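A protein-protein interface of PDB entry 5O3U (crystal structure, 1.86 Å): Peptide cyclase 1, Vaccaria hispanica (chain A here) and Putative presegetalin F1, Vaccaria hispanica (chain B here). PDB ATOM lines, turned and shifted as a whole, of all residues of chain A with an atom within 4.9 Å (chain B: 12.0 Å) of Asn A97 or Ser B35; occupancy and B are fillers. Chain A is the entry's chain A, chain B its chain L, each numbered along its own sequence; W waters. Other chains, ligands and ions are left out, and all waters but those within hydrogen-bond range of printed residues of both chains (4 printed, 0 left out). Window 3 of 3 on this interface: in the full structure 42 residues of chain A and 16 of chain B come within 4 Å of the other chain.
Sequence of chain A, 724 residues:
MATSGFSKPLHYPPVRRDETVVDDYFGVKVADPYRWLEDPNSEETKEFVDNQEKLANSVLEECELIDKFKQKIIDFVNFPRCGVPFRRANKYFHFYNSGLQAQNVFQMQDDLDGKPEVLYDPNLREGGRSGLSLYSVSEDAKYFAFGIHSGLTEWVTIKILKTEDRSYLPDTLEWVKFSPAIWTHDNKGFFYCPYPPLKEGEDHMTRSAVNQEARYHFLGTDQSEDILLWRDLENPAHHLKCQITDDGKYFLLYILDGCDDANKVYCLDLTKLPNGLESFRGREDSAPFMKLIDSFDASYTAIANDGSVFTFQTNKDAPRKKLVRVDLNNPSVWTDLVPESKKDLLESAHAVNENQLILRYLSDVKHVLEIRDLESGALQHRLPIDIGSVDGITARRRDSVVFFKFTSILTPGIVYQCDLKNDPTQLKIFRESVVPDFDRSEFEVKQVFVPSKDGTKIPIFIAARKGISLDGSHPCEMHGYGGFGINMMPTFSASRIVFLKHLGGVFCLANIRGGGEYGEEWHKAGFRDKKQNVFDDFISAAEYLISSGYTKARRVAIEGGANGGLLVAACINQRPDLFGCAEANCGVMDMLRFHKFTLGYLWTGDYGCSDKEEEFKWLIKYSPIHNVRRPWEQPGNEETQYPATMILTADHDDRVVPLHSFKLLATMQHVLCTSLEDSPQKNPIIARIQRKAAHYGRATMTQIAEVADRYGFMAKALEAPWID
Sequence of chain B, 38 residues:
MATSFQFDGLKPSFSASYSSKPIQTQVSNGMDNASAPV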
ATOM      1  N   PHE A  79      30.013  13.342  -0.025  1.00  0.00           N
ATOM      2  CA  PHE A  79      30.230  13.663  -1.423  1.00  0.00           C
ATOM      3  C   PHE A  79      29.425  14.911  -1.752  1.00  0.00           C
ATOM      4  O   PHE A  79      28.346  15.098  -1.210  1.00  0.00           O
ATOM      5  CB  PHE A  79      29.865  12.489  -2.372  1.00  0.00           C
ATOM      6  CG  PHE A  79      28.426  12.029  -2.289  1.00  0.00           C
ATOM      7  CD1 PHE A  79      27.420  12.618  -3.040  1.00  0.00           C
ATOM      8  CD2 PHE A  79      28.073  10.950  -1.464  1.00  0.00           C
ATOM      9  CE1 PHE A  79      26.120  12.201  -2.969  1.00  0.00           C
ATOM     10  CE2 PHE A  79      26.764  10.491  -1.393  1.00  0.00           C
ATOM     11  CZ  PHE A  79      25.779  11.149  -2.111  1.00  0.00           C
ATOM     12  N   PRO A  80      29.966  15.762  -2.644  1.00  0.00           N
ATOM     13  CA  PRO A  80      29.231  16.989  -2.931  1.00  0.00           C
ATOM     14  C   PRO A  80      27.933  16.742  -3.719  1.00  0.00           C
ATOM     15  O   PRO A  80      27.888  15.847  -4.540  1.00  0.00           O
ATOM     16  CB  PRO A  80      30.241  17.847  -3.707  1.00  0.00           C
ATOM     17  CG  PRO A  80      31.398  16.994  -4.034  1.00  0.00           C
ATOM     18  CD  PRO A  80      31.342  15.766  -3.173  1.00  0.00           C
ATOM     19  N   ARG A  81      26.895  17.503  -3.396  1.00  0.00           N
ATOM     20  CA  ARG A  81      25.561  17.356  -3.971  1.00  0.00           C
ATOM     21  C   ARG A  81      25.077  18.716  -4.447  1.00  0.00           C
ATOM     22  O   ARG A  81      24.976  19.681  -3.692  1.00  0.00           O
ATOM     23  CB  ARG A  81      24.590  16.820  -2.934  1.00  0.00           C
ATOM     24  CG  ARG A  81      24.884  15.361  -2.595  1.00  0.00           C
ATOM     25  CD  ARG A  81      23.953  14.817  -1.527  1.00  0.00           C
ATOM     26  NE  ARG A  81      24.102  15.445  -0.214  1.00  0.00           N
ATOM     27  CZ  ARG A  81      25.043  15.169   0.686  1.00  0.00           C
ATOM     28  NH1 ARG A  81      25.996  14.292   0.447  1.00  0.00           N
ATOM     29  NH2 ARG A  81      25.005  15.770   1.860  1.00  0.00           N
ATOM     30  N   PHE A  95      20.626  24.638  -4.752  1.00  0.00           N
ATOM     31  CA  PHE A  95      21.183  24.206  -3.468  1.00  0.00           C
ATOM     32  C   PHE A  95      22.459  23.428  -3.656  1.00  0.00           C
ATOM     33  O   PHE A  95      22.639  22.747  -4.656  1.00  0.00           O
ATOM     34  CB  PHE A  95      20.156  23.375  -2.694  1.00  0.00           C
ATOM     35  CG  PHE A  95      19.105  24.216  -2.040  1.00  0.00           C
ATOM     36  CD1 PHE A  95      19.374  24.884  -0.865  1.00  0.00           C
ATOM     37  CD2 PHE A  95      17.856  24.346  -2.615  1.00  0.00           C
ATOM     38  CE1 PHE A  95      18.413  25.683  -0.254  1.00  0.00           C
ATOM     39  CE2 PHE A  95      16.898  25.132  -2.029  1.00  0.00           C
ATOM     40  CZ  PHE A  95      17.161  25.805  -0.841  1.00  0.00           C
ATOM     41  N   TYR A  96      23.348  23.519  -2.669  1.00  0.00           N
ATOM     42  CA  TYR A  96      24.603  22.836  -2.681  1.00  0.00           C
ATOM     43  C   TYR A  96      24.940  22.356  -1.284  1.00  0.00           C
ATOM     44  O   TYR A  96      24.670  23.065  -0.319  1.00  0.00           O
ATOM     45  CB  TYR A  96      25.708  23.816  -3.127  1.00  0.00           C
ATOM     46  CG  TYR A  96      27.052  23.172  -3.201  1.00  0.00           C
ATOM     47  CD1 TYR A  96      27.337  22.215  -4.180  1.00  0.00           C
ATOM     48  CD2 TYR A  96      28.038  23.471  -2.261  1.00  0.00           C
ATOM     49  CE1 TYR A  96      28.589  21.600  -4.232  1.00  0.00           C
ATOM     50  CE2 TYR A  96      29.281  22.853  -2.306  1.00  0.00           C
ATOM     51  CZ  TYR A  96      29.550  21.931  -3.286  1.00  0.00           C
ATOM     52  OH  TYR A  96      30.779  21.330  -3.307  1.00  0.00           O
ATOM     53  N   ASN A  97      25.591  21.200  -1.206  1.00  0.00           N
ATOM     54  CA  ASN A  97      26.168  20.685   0.040  1.00  0.00           C
ATOM     55  C   ASN A  97      27.519  20.089  -0.328  1.00  0.00           C
ATOM     56  O   ASN A  97      27.614  19.223  -1.194  1.00  0.00           O
ATOM     57  CB  ASN A  97      25.267  19.614   0.655  1.00  0.00           C
ATOM     58  CG  ASN A  97      25.578  19.340   2.115  1.00  0.00           C
ATOM     59  OD1 ASN A  97      26.722  19.154   2.487  1.00  0.00           O
ATOM     60  ND2 ASN A  97      24.546  19.394   2.963  1.00  0.00           N
ATOM     61  N   SER A  98      28.581  20.512   0.352  1.00  0.00           N
ATOM     62  CA  SER A  98      29.890  19.965   0.094  1.00  0.00           C
ATOM     63  C   SER A  98      30.023  18.474   0.524  1.00  0.00           C
ATOM     64  O   SER A  98      30.993  17.806   0.156  1.00  0.00           O
ATOM     65  CB  SER A  98      30.956  20.830   0.764  1.00  0.00           C
ATOM     66  OG  SER A  98      30.782  20.824   2.149  1.00  0.00           O
ATOM     67  N   GLY A  99      29.045  17.978   1.281  1.00  0.00           N
ATOM     68  CA  GLY A  99      28.927  16.553   1.628  1.00  0.00           C
ATOM     69  C   GLY A  99      28.386  16.360   3.030  1.00  0.00           C
ATOM     70  O   GLY A  99      27.409  15.655   3.233  1.00  0.00           O
ATOM     71  N   LEU A 100      29.005  17.027   4.005  1.00  0.00           N
ATOM     72  CA  LEU A 100      28.611  16.867   5.390  1.00  0.00           C
ATOM     73  C   LEU A 100      28.207  18.165   6.081  1.00  0.00           C
ATOM     74  O   LEU A 100      28.257  18.254   7.305  1.00  0.00           O
ATOM     75  CB  LEU A 100      29.752  16.156   6.143  1.00  0.00           C
ATOM     76  CG  LEU A 100      29.990  14.708   5.706  1.00  0.00           C
ATOM     77  CD1 LEU A 100      31.295  14.193   6.304  1.00  0.00           C
ATOM     78  CD2 LEU A 100      28.833  13.820   6.075  1.00  0.00           C
ATOM     79  N   GLN A 101      27.771  19.163   5.305  1.00  0.00           N
ATOM     80  CA  GLN A 101      27.182  20.362   5.898  1.00  0.00           C
ATOM     81  C   GLN A 101      25.849  20.004   6.544  1.00  0.00           C
ATOM     82  O   GLN A 101      25.096  19.152   6.026  1.00  0.00           O
ATOM     83  CB  GLN A 101      26.999  21.494   4.859  1.00  0.00           C
ATOM     84  CG  GLN A 101      28.312  21.866   4.205  1.00  0.00           C
ATOM     85  CD  GLN A 101      28.198  23.020   3.267  1.00  0.00           C
ATOM     86  OE1 GLN A 101      28.047  22.839   2.052  1.00  0.00           O
ATOM     87  NE2 GLN A 101      28.278  24.217   3.816  1.00  0.00           N
ATOM     88  N   ALA A 102      25.567  20.621   7.689  1.00  0.00           N
ATOM     89  CA  ALA A 102      24.318  20.347   8.420  1.00  0.00           C
ATOM     90  C   ALA A 102      23.082  20.517   7.534  1.00  0.00           C
ATOM     91  O   ALA A 102      22.153  19.705   7.587  1.00  0.00           O
ATOM     92  CB  ALA A 102      24.197  21.213   9.654  1.00  0.00           C
ATOM     93  N   GLN A 103      23.097  21.582   6.736  1.00  0.00           N
ATOM     94  CA  GLN A 103      22.019  21.867   5.800  1.00  0.00           C
ATOM     95  C   GLN A 103      22.594  22.360   4.466  1.00  0.00           C
ATOM     96  O   GLN A 103      23.724  22.855   4.402  1.00  0.00           O
ATOM     97  CB  GLN A 103      21.111  22.968   6.370  1.00  0.00           C
ATOM     98  CG  GLN A 103      20.429  22.687   7.693  1.00  0.00           C
ATOM     99  CD  GLN A 103      19.412  21.558   7.659  1.00  0.00           C
ATOM    100  OE1 GLN A 103      18.959  21.137   6.586  1.00  0.00           O
ATOM    101  NE2 GLN A 103      19.064  21.047   8.836  1.00  0.00           N
ATOM    102  N   ASN A 104      21.770  22.275   3.424  1.00  0.00           N
ATOM    103  CA  ASN A 104      22.161  22.731   2.096  1.00  0.00           C
ATOM    104  C   ASN A 104      22.201  24.265   2.057  1.00  0.00           C
ATOM    105  O   ASN A 104      21.404  24.919   2.729  1.00  0.00           O
ATOM    106  CB  ASN A 104      21.200  22.206   1.026  1.00  0.00           C
ATOM    107  CG  ASN A 104      21.077  20.702   1.039  1.00  0.00           C
ATOM    108  OD1 ASN A 104      22.008  20.003   1.453  1.00  0.00           O
ATOM    109  ND2 ASN A 104      19.943  20.179   0.587  1.00  0.00           N
ATOM    110  N   ARG A 698      16.080  17.354   9.914  1.00  0.00           N
ATOM    111  CA  ARG A 698      17.194  17.302  10.767  1.00  0.00           C
ATOM    112  C   ARG A 698      18.542  17.498  10.043  1.00  0.00           C
ATOM    113  O   ARG A 698      18.747  17.097   8.896  1.00  0.00           O
ATOM    114  CB  ARG A 698      17.152  15.984  11.558  1.00  0.00           C
ATOM    115  CG  ARG A 698      15.938  15.925  12.492  1.00  0.00           C
ATOM    116  CD  ARG A 698      15.846  14.601  13.186  1.00  0.00           C
ATOM    117  NE  ARG A 698      14.451  14.265  13.498  1.00  0.00           N
ATOM    118  CZ  ARG A 698      14.082  13.196  14.192  1.00  0.00           C
ATOM    119  NH1 ARG A 698      14.990  12.358  14.682  1.00  0.00           N
ATOM    120  NH2 ARG A 698      12.791  12.954  14.415  1.00  0.00           N
ATOM    121  N   ALA A 699      19.432  18.134  10.774  1.00  0.00           N
ATOM    122  CA  ALA A 699      20.803  18.322  10.365  1.00  0.00           C
ATOM    123  C   ALA A 699      21.466  16.963  10.056  1.00  0.00           C
ATOM    124  O   ALA A 699      21.146  15.934  10.672  1.00  0.00           O
ATOM    125  CB  ALA A 699      21.551  19.036  11.472  1.00  0.00           C
ATOM    126  N   THR A 700      22.355  16.981   9.076  1.00  0.00           N
ATOM    127  CA  THR A 700      23.094  15.815   8.614  1.00  0.00           C
ATOM    128  C   THR A 700      23.577  14.881   9.735  1.00  0.00           C
ATOM    129  O   THR A 700      23.240  13.720   9.750  1.00  0.00           O
ATOM    130  CB  THR A 700      24.274  16.263   7.753  1.00  0.00           C
ATOM    131  OG1 THR A 700      23.754  16.937   6.587  1.00  0.00           O
ATOM    132  CG2 THR A 700      25.158  15.108   7.330  1.00  0.00           C
ATOM    133  N   GLN B  24       7.043  11.468   6.596  1.00  0.00           N
ATOM    134  CA  GLN B  24       8.324  12.043   7.071  1.00  0.00           C
ATOM    135  C   GLN B  24       9.247  12.352   5.881  1.00  0.00           C
ATOM    136  O   GLN B  24       8.758  12.706   4.822  1.00  0.00           O
ATOM    137  CB  GLN B  24       8.979  11.116   8.097  1.00  0.00           C
ATOM    138  CG  GLN B  24       9.375   9.725   7.608  1.00  0.00           C
ATOM    139  CD  GLN B  24      10.241   8.954   8.600  1.00  0.00           C
ATOM    140  OE1 GLN B  24      10.561   9.444   9.690  1.00  0.00           O
ATOM    141  NE2 GLN B  24      10.613   7.721   8.230  1.00  0.00           N
ATOM    142  N   THR B  25      10.576  12.311   6.050  1.00  0.00           N
ATOM    143  CA  THR B  25      11.503  12.025   4.917  1.00  0.00           C
ATOM    144  C   THR B  25      12.802  11.362   5.417  1.00  0.00           C
ATOM    145  O   THR B  25      13.869  11.981   5.484  1.00  0.00           O
ATOM    146  CB  THR B  25      11.816  13.261   4.023  1.00  0.00           C
ATOM    147  OG1 THR B  25      10.605  13.948   3.682  1.00  0.00           O
ATOM    148  CG2 THR B  25      12.529  12.828   2.708  1.00  0.00           C
ATOM    149  N   ASN B  33      14.330  19.233   0.201  1.00  0.00           N
ATOM    150  CA  ASN B  33      15.611  19.882   0.489  1.00  0.00           C
ATOM    151  C   ASN B  33      16.326  19.259   1.713  1.00  0.00           C
ATOM    152  O   ASN B  33      16.917  19.971   2.567  1.00  0.00           O
ATOM    153  CB  ASN B  33      15.394  21.391   0.680  1.00  0.00           C
ATOM    154  CG  ASN B  33      16.695  22.187   0.676  1.00  0.00           C
ATOM    155  OD1 ASN B  33      17.641  21.822  -0.009  1.00  0.00           O
ATOM    156  ND2 ASN B  33      16.749  23.262   1.459  1.00  0.00           N
ATOM    157  N   ALA B  34      16.292  17.927   1.774  1.00  0.00           N
ATOM    158  CA  ALA B  34      17.006  17.198   2.804  1.00  0.00           C
ATOM    159  C   ALA B  34      18.508  17.465   2.659  1.00  0.00           C
ATOM    160  O   ALA B  34      19.029  17.562   1.545  1.00  0.00           O
ATOM    161  CB  ALA B  34      16.718  15.690   2.730  1.00  0.00           C
ATOM    162  N   SER B  35      19.201  17.597   3.785  1.00  0.00           N
ATOM    163  CA  SER B  35      20.608  17.935   3.759  1.00  0.00           C
ATOM    164  C   SER B  35      21.483  16.821   3.172  1.00  0.00           C
ATOM    165  O   SER B  35      22.540  17.090   2.633  1.00  0.00           O
ATOM    166  CB  SER B  35      21.102  18.287   5.157  1.00  0.00           C
ATOM    167  OG  SER B  35      21.116  17.135   5.978  1.00  0.00           O
ATOM    168  N   ALA B  36      21.027  15.572   3.313  1.00  0.00           N
ATOM    169  CA  ALA B  36      21.823  14.432   2.916  1.00  0.00           C
ATOM    170  C   ALA B  36      20.919  13.228   2.717  1.00  0.00           C
ATOM    171  O   ALA B  36      19.927  13.107   3.404  1.00  0.00           O
ATOM    172  CB  ALA B  36      22.857  14.111   3.975  1.00  0.00           C
ATOM    173  N   PRO B  37      21.255  12.365   1.764  1.00  0.00           N
ATOM    174  CA  PRO B  37      20.449  11.149   1.508  1.00  0.00           C
ATOM    175  C   PRO B  37      20.970  10.061   2.459  1.00  0.00           C
ATOM    176  O   PRO B  37      21.666   9.140   2.033  1.00  0.00           O
ATOM    177  CB  PRO B  37      20.773  10.827   0.053  1.00  0.00           C
ATOM    178  CG  PRO B  37      22.161  11.316  -0.131  1.00  0.00           C
ATOM    179  CD  PRO B  37      22.285  12.559   0.734  1.00  0.00           C
ATOM    180  N   VAL B  38      20.646  10.203   3.734  1.00  0.00           N
ATOM    181  CA  VAL B  38      21.236   9.358   4.750  1.00  0.00           C
ATOM    182  C   VAL B  38      20.595   7.965   4.644  1.00  0.00           C
ATOM    183  O   VAL B  38      19.402   7.815   4.331  1.00  0.00           O
ATOM    184  CB  VAL B  38      21.062   9.943   6.166  1.00  0.00           C
ATOM    185  CG1 VAL B  38      21.652   9.007   7.214  1.00  0.00           C
ATOM    186  CG2 VAL B  38      21.727  11.294   6.276  1.00  0.00           C
ATOM    187  OXT VAL B  38      21.294   6.964   4.841  1.00  0.00           O
HETATM  188  O   HOH W   1      19.063  21.250   3.898  1.00  0.00           O
HETATM  189  O   HOH W   2      18.767  24.190   3.432  1.00  0.00           O
HETATM  190  O   HOH W   3      17.889  17.930   6.394  1.00  0.00           O
HETATM  191  O   HOH W   4      22.208  17.838  -0.190  1.00  0.00           O
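The guanidinium group (NH2) of Arg A81 lies within hydrogen-bond range of the backbone carbonyl oxygen (O) of Ser B35, at 2.9 Å.
The side-chain amide nitrogen (ND2) of Asn A97 sits at hydrogen-bond distance from the backbone carbonyl oxygen (O) of Ser B35 (3.1 Å).
The backbone carbonyl oxygen (O) of Ala A102 lies close to the side-chain hydroxyl (OG) of Ser B35, at 3.2 Å.
ND2 of Asn A104 is in hydrogen-bond range of OD1 of Asn B33 (2.9 Å).
ND2 of Asn A104 lies within hydrogen-bond range of O of Ala B34.
OD1 of Asn A104 sits close to O of Ser B35.
OG1 of Thr A700 lies within hydrogen-bond range of OG of Ser B35, at 2.7 Å.
The backbone NH (N) of Arg A81 is in hydrogen-bond range of the backbone carbonyl oxygen (O) of Asn A97 (2.9 Å).
The guanidinium group (NH2) of Arg A81 is in hydrogen-bond range of the backbone carbonyl oxygen (O) of Gly A99 (2.8 Å).
OD1 of Asn A97 is in hydrogen-bond range of N of Leu A100.
ND2 of Asn A97 lies within hydrogen-bond range of OD1 of Asn A104.
The backbone carbonyl oxygen of Gln A101 is in hydrogen-bond range of the side-chain hydroxyl of Thr A700.
The backbone NH of Thr A700 lies within hydrogen-bond range of the backbone carbonyl oxygen of Ala A102.
Among the printed residues, pairs that only touch across the chains: Arg A81 with Ala B36 (3.4 Å), Arg A81 with Pro B37 (3.5 Å), Phe A95 with Asn B33 (3.4 Å), Gln A103 with Ser B35 (3.8 Å), Arg A698 with Ser B35 (3.8 Å) and Thr A700 with Ala B36 (3.95 Å).
Asn A97 touches just one residue of chain B: Ser B35 (3.1 Å).
Of the printed residues of chain A, Ser B35 touches Arg A81 (2.9 Å), Asn A97 (3.1 Å), Ala A102 (3.0 Å), Gln A103 (3.8 Å), Asn A104 (3.2 Å), Arg A698 (3.8 Å) and Thr A700 (2.7 Å).
No residue of chain B comes within 4 Å of Pro A80.
Arg A81 touches three residues of chain B.
No residue of chain B comes within 4 Å of Gly A99.
No residue of chain B comes within 4 Å of Leu A100.
Of chain B, only Ser B35 (3.0 Å) comes within 4 Å of Ala A102.
Of chain B, only Ser B35 (3.8 Å) comes within 4 Å of Gln A103.
Asn A104 touches just these residues of chain B: Asn B33, Ala B34 and Ser B35.
No residue of chain B comes within 4 Å of Ala A699.
Of chain B, only Ser B35 (2.7 Å) and Ala B36 (3.95 Å) come within 4 Å of Thr A700.
Printed residues of chain B within 4 Å of Arg A698: Ser B35.
Of the printed residues of chain A, Asn B33 touches Phe A95 and Asn A104.
Phe A79 touches none of the printed residues of chain B.
Val B38 touches none of the printed residues of chain A.
The nearest residue of chain B that does not touch Asn A97 is Ala B36 (5.2 Å).
The nearest residue of chain A that does not touch Ser B35 is Ala A699 (4.1 Å).
The nearest printed residue of chain A that does not touch Ala B36 is Gly A99 (4.9 Å).
Hydrophobic or aromatic side chains of chain A that line the printed part of chain B: Phe A95.
Of the 8 printed residues of chain B, 5 touch a printed residue of chain A.
Hydrophobic or aromatic side chains of chain B that line the printed part of chain A: Ala B36 and Pro B37.
Water W1 lies within hydrogen-bond range of the side-chain amide oxygen (OE1) of Gln A103, the backbone carbonyl oxygen (O) of Asn B33 and the backbone NH (N) of Asn A104.
Water W4 lies within hydrogen-bond range of OD1 of Asn A104 (2.7 Å), O of Ser B35 (2.9 Å) and NE of Arg A81 (3.1 Å).
Water W3 lies within hydrogen-bond range of the backbone carbonyl oxygen of Arg A698 (2.8 Å), the backbone NH of Ser B35 (2.9 Å) and the side-chain amide oxygen of Gln A103 (3.4 Å).
Water W2 lies within hydrogen-bond range of the backbone carbonyl oxygen of Asn A104 and the side-chain amide nitrogen of Asn B33.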
